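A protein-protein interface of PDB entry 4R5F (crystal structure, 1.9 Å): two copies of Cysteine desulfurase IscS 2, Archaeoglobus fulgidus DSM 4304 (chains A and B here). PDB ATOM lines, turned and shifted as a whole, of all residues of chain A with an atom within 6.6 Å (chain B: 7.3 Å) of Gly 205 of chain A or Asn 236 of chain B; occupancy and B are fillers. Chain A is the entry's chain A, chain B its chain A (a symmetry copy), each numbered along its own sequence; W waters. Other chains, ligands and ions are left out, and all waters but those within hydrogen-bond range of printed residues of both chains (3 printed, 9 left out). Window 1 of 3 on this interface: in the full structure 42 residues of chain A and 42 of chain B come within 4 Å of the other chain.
The side-chain amide nitrogen (ND2) of Asn 236 of chain A sits at hydrogen-bond distance from the side-chain hydroxyl (OG) of Ser 239 of chain A (2.8 Å).
The backbone NH (N) of Val 206 of chain B is in hydrogen-bond range of the backbone carbonyl oxygen (O) of Ser 67 of chain B.
The side-chain amide nitrogen (ND2) of Asn 236 of chain B sits at hydrogen-bond distance from the side-chain hydroxyl (OG) of Ser 239 of chain B (2.8 Å).
The backbone carbonyl oxygen (O) of Ser 67 of chain A sits at hydrogen-bond distance from the backbone NH (N) of Val 206 of chain A (3.3 Å).
Among the printed residues, pairs that only touch across the chains: Ser 67 of chain A with Ser 67 of chain B, Ser 67 of chain A with Arg 231 of chain B, Lys 204 of chain A with Glu 235 of chain B, Gly 205 of chain A with Asn 236 of chain B, Arg 231 of chain A with Ser 67 of chain B and Asn 236 of chain A with Gly 205 of chain B.
Ser 67 of chain B touches its own counterpart, Ser 67 of chain A.
Ser 67 of chain A touches Arg 231 of chain B, and with the chains exchanged Arg 231 of chain A touches Ser 67 of chain B.
Lys 204 of chain A touches Asn 236 of chain B, and with the chains exchanged Asn 236 of chain A touches Lys 204 of chain B.
Gly 205 of chain A touches Asn 236 of chain B, and with the chains exchanged Asn 236 of chain A touches Gly 205 of chain B.
9 positions are printed for both chains.
Of the 8 pairs that touch across the chains among the printed residues, 7 have their exchanged pair printed and touching as well.
Of the printed residues of chain B, Ser 67 of chain A touches Ser 67 (3.6 Å) and Arg 231 (3.6 Å).
Of chain B, only Asn 236 (3.3 Å) comes within 4 Å of Gly 205 of chain A.
Of the printed residues of chain B, Asn 236 of chain A touches Lys 204 (3.5 Å) and Gly 205 (3.3 Å).
Of the printed residues of chain A, Gly 205 of chain B touches Asn 236.
Of the printed residues of chain A, Arg 231 of chain B touches Ser 67 (3.6 Å).
The nearest residue of chain B that does not touch Gly 205 of chain A is Gly 205 of chain B (4.9 Å).
The backbone carbonyl oxygen (O) of Lys 204 of chain A lies within hydrogen-bond range of the side-chain amide nitrogen (ND2) of Asn 236 of chain B.
ND2 of Asn 236 of chain A is in hydrogen-bond range of O of Lys 204 of chain B, at 3.5 Å.
Of the 22 printed residues of chain B, 6 touch a printed residue of chain A.
Printed residues of chain B that touch a printed residue of chain A: Ser 67, Lys 204, Gly 205, Arg 231, Glu 235 and Asn 236.
Among the printed residues, no Asp or Glu carboxylate lies within 4 Å of a Lys or Arg side-chain nitrogen of the other chain.
Water W3 lies within hydrogen-bond range of the backbone carbonyl oxygen of Lys 204 of chain B, the side-chain hydroxyl of Ser 239 of chain B, the side-chain amide nitrogen of Asn 236 of chain A and the side-chain hydroxyl of Ser 239 of chain A.
Water W2 lies within hydrogen-bond range of the backbone carbonyl oxygen (O) of Lys 204 of chain A (2.7 Å), the side-chain hydroxyl (OG) of Ser 239 of chain A (2.7 Å), the side-chain amide nitrogen (ND2) of Asn 236 of chain B (2.7 Å) and the side-chain hydroxyl (OG) of Ser 239 of chain B (3.5 Å).
Water W1 lies within hydrogen-bond range of O of Glu 235 of chain B (2.7 Å) and NZ of Lys 204 of chain A (2.8 Å).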
ATOM      1  N   THR A  66      17.271  -8.748 -28.364  1.00  0.00           N
ATOM      2  CA  THR A  66      16.865  -9.682 -27.340  1.00  0.00           C
ATOM      3  C   THR A  66      17.272  -9.171 -25.965  1.00  0.00           C
ATOM      4  O   THR A  66      17.866  -8.105 -25.824  1.00  0.00           O
ATOM      5  CB  THR A  66      17.527 -11.047 -27.544  1.00  0.00           C
ATOM      6  OG1 THR A  66      18.939 -10.911 -27.297  1.00  0.00           O
ATOM      7  CG2 THR A  66      17.286 -11.546 -28.926  1.00  0.00           C
ATOM      8  N   SER A  67      16.960  -9.951 -24.948  1.00  0.00           N
ATOM      9  CA  SER A  67      17.394  -9.633 -23.601  1.00  0.00           C
ATOM     10  C   SER A  67      18.844 -10.045 -23.340  1.00  0.00           C
ATOM     11  O   SER A  67      19.304  -9.906 -22.219  1.00  0.00           O
ATOM     12  CB  SER A  67      16.481 -10.328 -22.583  1.00  0.00           C
ATOM     13  OG  SER A  67      16.625 -11.737 -22.707  1.00  0.00           O
ATOM     14  N   GLY A  68      19.549 -10.558 -24.347  1.00  0.00           N
ATOM     15  CA  GLY A  68      20.944 -10.951 -24.186  1.00  0.00           C
ATOM     16  C   GLY A  68      21.321 -12.156 -25.030  1.00  0.00           C
ATOM     17  O   GLY A  68      20.527 -12.695 -25.807  1.00  0.00           O
ATOM     18  N   SER A 197      25.569  -7.517 -25.729  1.00  0.00           N
ATOM     19  CA  SER A 197      25.829  -6.122 -25.459  1.00  0.00           C
ATOM     20  C   SER A 197      26.906  -5.911 -24.403  1.00  0.00           C
ATOM     21  O   SER A 197      27.875  -5.163 -24.617  1.00  0.00           O
ATOM     22  CB  SER A 197      24.542  -5.419 -25.009  1.00  0.00           C
ATOM     23  OG  SER A 197      24.812  -4.105 -24.568  1.00  0.00           O
ATOM     24  N   ASN A 198      26.777  -6.579 -23.264  1.00  0.00           N
ATOM     25  CA  ASN A 198      27.736  -6.323 -22.206  1.00  0.00           C
ATOM     26  C   ASN A 198      29.164  -6.767 -22.550  1.00  0.00           C
ATOM     27  O   ASN A 198      30.118  -6.205 -22.022  1.00  0.00           O
ATOM     28  CB  ASN A 198      27.321  -6.982 -20.918  1.00  0.00           C
ATOM     29  CG  ASN A 198      28.223  -6.588 -19.776  1.00  0.00           C
ATOM     30  OD1 ASN A 198      28.837  -7.439 -19.156  1.00  0.00           O
ATOM     31  ND2 ASN A 198      28.338  -5.291 -19.514  1.00  0.00           N
ATOM     32  N   PRO A 203      25.297  -2.101 -21.903  1.00  0.00           N
ATOM     33  CA  PRO A 203      24.492  -2.570 -20.771  1.00  0.00           C
ATOM     34  C   PRO A 203      24.180  -4.051 -20.834  1.00  0.00           C
ATOM     35  O   PRO A 203      24.011  -4.623 -21.902  1.00  0.00           O
ATOM     36  CB  PRO A 203      23.209  -1.747 -20.883  1.00  0.00           C
ATOM     37  CG  PRO A 203      23.102  -1.394 -22.395  1.00  0.00           C
ATOM     38  CD  PRO A 203      24.548  -1.235 -22.842  1.00  0.00           C
ATOM     39  N   LYS A 204      24.129  -4.665 -19.653  1.00  0.00           N
ATOM     40  CA  LYS A 204      23.635  -6.009 -19.480  1.00  0.00           C
ATOM     41  C   LYS A 204      22.162  -5.980 -19.860  1.00  0.00           C
ATOM     42  O   LYS A 204      21.563  -4.922 -19.892  1.00  0.00           O
ATOM     43  CB  LYS A 204      23.815  -6.471 -18.047  1.00  0.00           C
ATOM     44  CG  LYS A 204      25.266  -6.699 -17.665  1.00  0.00           C
ATOM     45  CD  LYS A 204      25.389  -6.938 -16.150  1.00  0.00           C
ATOM     46  CE  LYS A 204      26.859  -7.072 -15.753  1.00  0.00           C
ATOM     47  NZ  LYS A 204      27.007  -7.467 -14.313  1.00  0.00           N
ATOM     48  N   GLY A 205      21.583  -7.137 -20.133  1.00  0.00           N
ATOM     49  CA  GLY A 205      20.138  -7.230 -20.262  1.00  0.00           C
ATOM     50  C   GLY A 205      19.632  -7.002 -21.683  1.00  0.00           C
ATOM     51  O   GLY A 205      18.412  -6.945 -21.914  1.00  0.00           O
ATOM     52  N   VAL A 206      20.565  -6.882 -22.625  1.00  0.00           N
ATOM     53  CA  VAL A 206      20.229  -6.741 -24.052  1.00  0.00           C
ATOM     54  C   VAL A 206      21.299  -7.480 -24.881  1.00  0.00           C
ATOM     55  O   VAL A 206      22.435  -7.715 -24.421  1.00  0.00           O
ATOM     56  CB  VAL A 206      20.094  -5.255 -24.461  1.00  0.00           C
ATOM     57  CG1 VAL A 206      21.411  -4.521 -24.350  1.00  0.00           C
ATOM     58  CG2 VAL A 206      19.469  -5.108 -25.840  1.00  0.00           C
ATOM     59  N   GLY A 207      20.887  -7.974 -26.031  1.00  0.00           N
ATOM     60  CA  GLY A 207      21.795  -8.487 -27.032  1.00  0.00           C
ATOM     61  C   GLY A 207      21.072  -8.616 -28.344  1.00  0.00           C
ATOM     62  O   GLY A 207      20.031  -8.012 -28.519  1.00  0.00           O
ATOM     63  N   ARG A 231      10.197 -11.298 -31.875  1.00  0.00           N
ATOM     64  CA  ARG A 231      10.521 -11.154 -30.458  1.00  0.00           C
ATOM     65  C   ARG A 231       9.662 -10.071 -29.816  1.00  0.00           C
ATOM     66  O   ARG A 231      10.051  -8.887 -29.788  1.00  0.00           O
ATOM     67  CB  ARG A 231      12.010 -10.820 -30.286  1.00  0.00           C
ATOM     68  CG  ARG A 231      12.555 -11.006 -28.862  1.00  0.00           C
ATOM     69  CD  ARG A 231      12.350  -9.756 -27.993  1.00  0.00           C
ATOM     70  NE  ARG A 231      12.980  -9.879 -26.677  1.00  0.00           N
ATOM     71  CZ  ARG A 231      12.952  -8.923 -25.756  1.00  0.00           C
ATOM     72  NH1 ARG A 231      12.332  -7.766 -26.021  1.00  0.00           N
ATOM     73  NH2 ARG A 231      13.528  -9.127 -24.573  1.00  0.00           N
ATOM     74  N   ASN A 236      13.078  -2.089 -24.997  1.00  0.00           N
ATOM     75  CA  ASN A 236      13.885  -1.501 -23.942  1.00  0.00           C
ATOM     76  C   ASN A 236      14.805  -0.501 -24.586  1.00  0.00           C
ATOM     77  O   ASN A 236      15.970  -0.802 -24.899  1.00  0.00           O
ATOM     78  CB  ASN A 236      14.675  -2.593 -23.164  1.00  0.00           C
ATOM     79  CG  ASN A 236      15.531  -2.019 -22.081  1.00  0.00           C
ATOM     80  OD1 ASN A 236      15.585  -0.813 -21.880  1.00  0.00           O
ATOM     81  ND2 ASN A 236      16.235  -2.881 -21.377  1.00  0.00           N
ATOM     82  N   SER A 239      18.462   0.425 -23.210  1.00  0.00           N
ATOM     83  CA  SER A 239      19.484  -0.613 -23.343  1.00  0.00           C
ATOM     84  C   SER A 239      19.863  -0.807 -24.823  1.00  0.00           C
ATOM     85  O   SER A 239      21.016  -0.996 -25.134  1.00  0.00           O
ATOM     86  CB  SER A 239      19.026  -1.936 -22.744  1.00  0.00           C
ATOM     87  OG  SER A 239      18.795  -1.788 -21.361  1.00  0.00           O
ATOM     88  N   MET B  20      20.585   2.500  -9.415  1.00  0.00           N
ATOM     89  CA  MET B  20      21.025   1.589 -10.476  1.00  0.00           C
ATOM     90  C   MET B  20      22.450   1.778 -10.869  1.00  0.00           C
ATOM     91  O   MET B  20      23.125   0.825 -11.212  1.00  0.00           O
ATOM     92  CB  MET B  20      20.211   1.793 -11.747  1.00  0.00           C
ATOM     93  CG  MET B  20      18.838   1.213 -11.683  1.00  0.00           C
ATOM     94  SD  MET B  20      17.901   1.656 -13.125  1.00  0.00           S
ATOM     95  CE  MET B  20      18.766   0.715 -14.379  1.00  0.00           C
ATOM     96  N   MET B  24      26.205  -0.376 -12.891  1.00  0.00           N
ATOM     97  CA  MET B  24      26.568  -0.298 -14.296  1.00  0.00           C
ATOM     98  C   MET B  24      28.076  -0.392 -14.441  1.00  0.00           C
ATOM     99  O   MET B  24      28.590  -1.276 -15.135  1.00  0.00           O
ATOM    100  CB  MET B  24      26.067   1.008 -14.924  1.00  0.00           C
ATOM    101  CG  MET B  24      24.561   1.159 -14.941  1.00  0.00           C
ATOM    102  SD  MET B  24      23.824   0.225 -16.280  1.00  0.00           S
ATOM    103  CE  MET B  24      22.102   0.717 -16.104  1.00  0.00           C
ATOM    104  N   PRO B  31      26.616 -12.210 -10.543  1.00  0.00           N
ATOM    105  CA  PRO B  31      26.274 -12.883  -9.271  1.00  0.00           C
ATOM    106  C   PRO B  31      26.716 -14.336  -9.171  1.00  0.00           C
ATOM    107  O   PRO B  31      26.726 -14.911  -8.070  1.00  0.00           O
ATOM    108  CB  PRO B  31      24.736 -12.825  -9.240  1.00  0.00           C
ATOM    109  CG  PRO B  31      24.364 -11.675 -10.072  1.00  0.00           C
ATOM    110  CD  PRO B  31      25.405 -11.660 -11.200  1.00  0.00           C
ATOM    111  N   VAL B  45      21.124  -8.509  -5.863  1.00  0.00           N
ATOM    112  CA  VAL B  45      20.004  -9.191  -6.490  1.00  0.00           C
ATOM    113  C   VAL B  45      19.029  -9.746  -5.456  1.00  0.00           C
ATOM    114  O   VAL B  45      17.783  -9.631  -5.632  1.00  0.00           O
ATOM    115  CB  VAL B  45      20.487 -10.307  -7.441  1.00  0.00           C
ATOM    116  CG1 VAL B  45      19.341 -11.220  -7.889  1.00  0.00           C
ATOM    117  CG2 VAL B  45      21.183  -9.694  -8.669  1.00  0.00           C
ATOM    118  N   PHE B  65      12.887 -13.242 -11.893  1.00  0.00           N
ATOM    119  CA  PHE B  65      13.163 -12.112 -12.767  1.00  0.00           C
ATOM    120  C   PHE B  65      13.155 -12.474 -14.252  1.00  0.00           C
ATOM    121  O   PHE B  65      13.646 -13.519 -14.681  1.00  0.00           O
ATOM    122  CB  PHE B  65      14.501 -11.468 -12.419  1.00  0.00           C
ATOM    123  CG  PHE B  65      14.493 -10.735 -11.102  1.00  0.00           C
ATOM    124  CD1 PHE B  65      13.610  -9.677 -10.889  1.00  0.00           C
ATOM    125  CD2 PHE B  65      15.375 -11.089 -10.073  1.00  0.00           C
ATOM    126  CE1 PHE B  65      13.581  -9.001  -9.677  1.00  0.00           C
ATOM    127  CE2 PHE B  65      15.356 -10.421  -8.858  1.00  0.00           C
ATOM    128  CZ  PHE B  65      14.427  -9.375  -8.646  1.00  0.00           C
ATOM    129  N   THR B  66      12.581 -11.572 -15.029  1.00  0.00           N
ATOM    130  CA  THR B  66      12.484 -11.732 -16.461  1.00  0.00           C
ATOM    131  C   THR B  66      12.901 -10.448 -17.166  1.00  0.00           C
ATOM    132  O   THR B  66      13.256  -9.453 -16.538  1.00  0.00           O
ATOM    133  CB  THR B  66      11.049 -12.049 -16.886  1.00  0.00           C
ATOM    134  OG1 THR B  66      10.233 -10.885 -16.647  1.00  0.00           O
ATOM    135  CG2 THR B  66      10.523 -13.217 -16.126  1.00  0.00           C
ATOM    136  N   SER B  67      12.844 -10.472 -18.484  1.00  0.00           N
ATOM    137  CA  SER B  67      13.105  -9.280 -19.266  1.00  0.00           C
ATOM    138  C   SER B  67      11.894  -8.346 -19.333  1.00  0.00           C
ATOM    139  O   SER B  67      11.958  -7.346 -20.028  1.00  0.00           O
ATOM    140  CB  SER B  67      13.518  -9.672 -20.690  1.00  0.00           C
ATOM    141  OG  SER B  67      12.428 -10.319 -21.334  1.00  0.00           O
ATOM    142  N   PRO B 203      13.236   0.658 -14.438  1.00  0.00           N
ATOM    143  CA  PRO B 203      13.757   0.510 -15.801  1.00  0.00           C
ATOM    144  C   PRO B 203      12.947  -0.449 -16.649  1.00  0.00           C
ATOM    145  O   PRO B 203      12.402  -1.429 -16.161  1.00  0.00           O
ATOM    146  CB  PRO B 203      15.171  -0.029 -15.583  1.00  0.00           C
ATOM    147  CG  PRO B 203      15.100  -0.770 -14.215  1.00  0.00           C
ATOM    148  CD  PRO B 203      14.101   0.044 -13.406  1.00  0.00           C
ATOM    149  N   LYS B 204      12.865  -0.125 -17.939  1.00  0.00           N
ATOM    150  CA  LYS B 204      12.333  -1.011 -18.945  1.00  0.00           C
ATOM    151  C   LYS B 204      13.268  -2.211 -19.002  1.00  0.00           C
ATOM    152  O   LYS B 204      14.391  -2.128 -18.543  1.00  0.00           O
ATOM    153  CB  LYS B 204      12.259  -0.318 -20.291  1.00  0.00           C
ATOM    154  CG  LYS B 204      11.205   0.772 -20.352  1.00  0.00           C
ATOM    155  CD  LYS B 204      11.343   1.578 -21.655  1.00  0.00           C
ATOM    156  CE  LYS B 204      10.342   2.734 -21.670  1.00  0.00           C
ATOM    157  NZ  LYS B 204      10.338   3.442 -22.993  1.00  0.00           N
ATOM    158  N   GLY B 205      12.809  -3.311 -19.572  1.00  0.00           N
ATOM    159  CA  GLY B 205      13.705  -4.411 -19.889  1.00  0.00           C
ATOM    160  C   GLY B 205      13.847  -5.432 -18.764  1.00  0.00           C
ATOM    161  O   GLY B 205      14.664  -6.363 -18.860  1.00  0.00           O
ATOM    162  N   VAL B 206      13.048  -5.260 -17.713  1.00  0.00           N
ATOM    163  CA  VAL B 206      13.012  -6.210 -16.588  1.00  0.00           C
ATOM    164  C   VAL B 206      11.563  -6.295 -16.066  1.00  0.00           C
ATOM    165  O   VAL B 206      10.739  -5.380 -16.273  1.00  0.00           O
ATOM    166  CB  VAL B 206      14.012  -5.814 -15.477  1.00  0.00           C
ATOM    167  CG1 VAL B 206      13.635  -4.504 -14.823  1.00  0.00           C
ATOM    168  CG2 VAL B 206      14.191  -6.932 -14.460  1.00  0.00           C
ATOM    169  N   ARG B 231      14.811 -19.555 -15.452  1.00  0.00           N
ATOM    170  CA  ARG B 231      15.046 -18.481 -16.415  1.00  0.00           C
ATOM    171  C   ARG B 231      16.537 -18.191 -16.544  1.00  0.00           C
ATOM    172  O   ARG B 231      17.083 -17.342 -15.812  1.00  0.00           O
ATOM    173  CB  ARG B 231      14.295 -17.212 -15.988  1.00  0.00           C
ATOM    174  CG  ARG B 231      14.156 -16.143 -17.082  1.00  0.00           C
ATOM    175  CD  ARG B 231      15.369 -15.201 -17.132  1.00  0.00           C
ATOM    176  NE  ARG B 231      15.187 -14.104 -18.085  1.00  0.00           N
ATOM    177  CZ  ARG B 231      16.091 -13.155 -18.294  1.00  0.00           C
ATOM    178  NH1 ARG B 231      17.237 -13.168 -17.602  1.00  0.00           N
ATOM    179  NH2 ARG B 231      15.858 -12.206 -19.198  1.00  0.00           N
ATOM    180  N   GLY B 233      20.319 -17.112 -17.999  1.00  0.00           N
ATOM    181  CA  GLY B 233      20.962 -15.925 -18.534  1.00  0.00           C
ATOM    182  C   GLY B 233      21.619 -15.186 -17.385  1.00  0.00           C
ATOM    183  O   GLY B 233      21.047 -15.145 -16.304  1.00  0.00           O
ATOM    184  N   SER B 234      22.792 -14.594 -17.631  1.00  0.00           N
ATOM    185  CA  SER B 234      23.512 -13.793 -16.641  1.00  0.00           C
ATOM    186  C   SER B 234      22.626 -12.673 -16.110  1.00  0.00           C
ATOM    187  O   SER B 234      22.000 -11.977 -16.895  1.00  0.00           O
ATOM    188  CB  SER B 234      24.769 -13.184 -17.253  1.00  0.00           C
ATOM    189  OG  SER B 234      25.698 -14.200 -17.567  1.00  0.00           O
ATOM    190  N   GLU B 235      22.596 -12.456 -14.794  1.00  0.00           N
ATOM    191  CA  GLU B 235      21.637 -11.499 -14.258  1.00  0.00           C
ATOM    192  C   GLU B 235      21.912 -10.090 -14.725  1.00  0.00           C
ATOM    193  O   GLU B 235      23.043  -9.651 -14.729  1.00  0.00           O
ATOM    194  CB  GLU B 235      21.622 -11.540 -12.731  1.00  0.00           C
ATOM    195  CG  GLU B 235      21.125 -12.820 -12.218  1.00  0.00           C
ATOM    196  CD  GLU B 235      22.187 -13.910 -12.067  1.00  0.00           C
ATOM    197  OE1 GLU B 235      23.301 -13.819 -12.660  1.00  0.00           O
ATOM    198  OE2 GLU B 235      21.872 -14.865 -11.322  1.00  0.00           O
ATOM    199  N   ASN B 236      20.850  -9.366 -15.085  1.00  0.00           N
ATOM    200  CA  ASN B 236      20.965  -7.951 -15.391  1.00  0.00           C
ATOM    201  C   ASN B 236      20.849  -7.201 -14.093  1.00  0.00           C
ATOM    202  O   ASN B 236      19.765  -6.725 -13.715  1.00  0.00           O
ATOM    203  CB  ASN B 236      19.877  -7.508 -16.411  1.00  0.00           C
ATOM    204  CG  ASN B 236      19.955  -6.050 -16.736  1.00  0.00           C
ATOM    205  OD1 ASN B 236      20.789  -5.323 -16.215  1.00  0.00           O
ATOM    206  ND2 ASN B 236      19.063  -5.596 -17.591  1.00  0.00           N
ATOM    207  N   VAL B 237      21.971  -7.120 -13.384  1.00  0.00           N
ATOM    208  CA  VAL B 237      21.960  -6.637 -12.015  1.00  0.00           C
ATOM    209  C   VAL B 237      21.470  -5.176 -11.899  1.00  0.00           C
ATOM    210  O   VAL B 237      20.678  -4.869 -11.010  1.00  0.00           O
ATOM    211  CB  VAL B 237      23.345  -6.778 -11.384  1.00  0.00           C
ATOM    212  CG1 VAL B 237      23.310  -6.271  -9.974  1.00  0.00           C
ATOM    213  CG2 VAL B 237      23.791  -8.282 -11.424  1.00  0.00           C
ATOM    214  N   PRO B 238      21.928  -4.281 -12.793  1.00  0.00           N
ATOM    215  CA  PRO B 238      21.474  -2.903 -12.655  1.00  0.00           C
ATOM    216  C   PRO B 238      19.937  -2.791 -12.809  1.00  0.00           C
ATOM    217  O   PRO B 238      19.349  -2.089 -12.007  1.00  0.00           O
ATOM    218  CB  PRO B 238      22.245  -2.175 -13.751  1.00  0.00           C
ATOM    219  CG  PRO B 238      23.484  -3.029 -13.973  1.00  0.00           C
ATOM    220  CD  PRO B 238      22.962  -4.417 -13.835  1.00  0.00           C
ATOM    221  N   SER B 239      19.318  -3.505 -13.743  1.00  0.00           N
ATOM    222  CA  SER B 239      17.876  -3.382 -13.951  1.00  0.00           C
ATOM    223  C   SER B 239      17.107  -4.036 -12.788  1.00  0.00           C
ATOM    224  O   SER B 239      16.107  -3.513 -12.353  1.00  0.00           O
ATOM    225  CB  SER B 239      17.442  -3.997 -15.275  1.00  0.00           C
ATOM    226  OG  SER B 239      18.053  -3.319 -16.349  1.00  0.00           O
ATOM    227  N   ILE B 240      17.635  -5.140 -12.269  1.00  0.00           N
ATOM    228  CA  ILE B 240      17.066  -5.817 -11.124  1.00  0.00           C
ATOM    229  C   ILE B 240      17.081  -4.880  -9.920  1.00  0.00           C
ATOM    230  O   ILE B 240      16.082  -4.731  -9.234  1.00  0.00           O
ATOM    231  CB  ILE B 240      17.840  -7.134 -10.826  1.00  0.00           C
ATOM    232  CG1 ILE B 240      17.435  -8.172 -11.867  1.00  0.00           C
ATOM    233  CG2 ILE B 240      17.533  -7.612  -9.419  1.00  0.00           C
ATOM    234  CD1 ILE B 240      18.367  -9.403 -11.994  1.00  0.00           C
ATOM    235  N   VAL B 241      18.207  -4.215  -9.692  1.00  0.00           N
ATOM    236  CA  VAL B 241      18.313  -3.298  -8.585  1.00  0.00           C
ATOM    237  C   VAL B 241      17.322  -2.130  -8.751  1.00  0.00           C
ATOM    238  O   VAL B 241      16.711  -1.703  -7.792  1.00  0.00           O
ATOM    239  CB  VAL B 241      19.742  -2.780  -8.444  1.00  0.00           C
ATOM    240  CG1 VAL B 241      19.803  -1.609  -7.510  1.00  0.00           C
ATOM    241  CG2 VAL B 241      20.696  -3.934  -7.932  1.00  0.00           C
ATOM    242  N   GLY B 242      17.203  -1.592  -9.963  1.00  0.00           N
ATOM    243  CA  GLY B 242      16.261  -0.508 -10.172  1.00  0.00           C
ATOM    244  C   GLY B 242      14.832  -0.961  -9.896  1.00  0.00           C
ATOM    245  O   GLY B 242      14.062  -0.253  -9.272  1.00  0.00           O
HETATM  246  O   HOH W   1      25.744 -10.006 -14.428  1.00  0.00           O
HETATM  247  O   HOH W   2      19.194  -3.768 -19.594  1.00  0.00           O
HETATM  248  O   HOH W   3      16.880  -3.021 -18.744  1.00  0.00           O
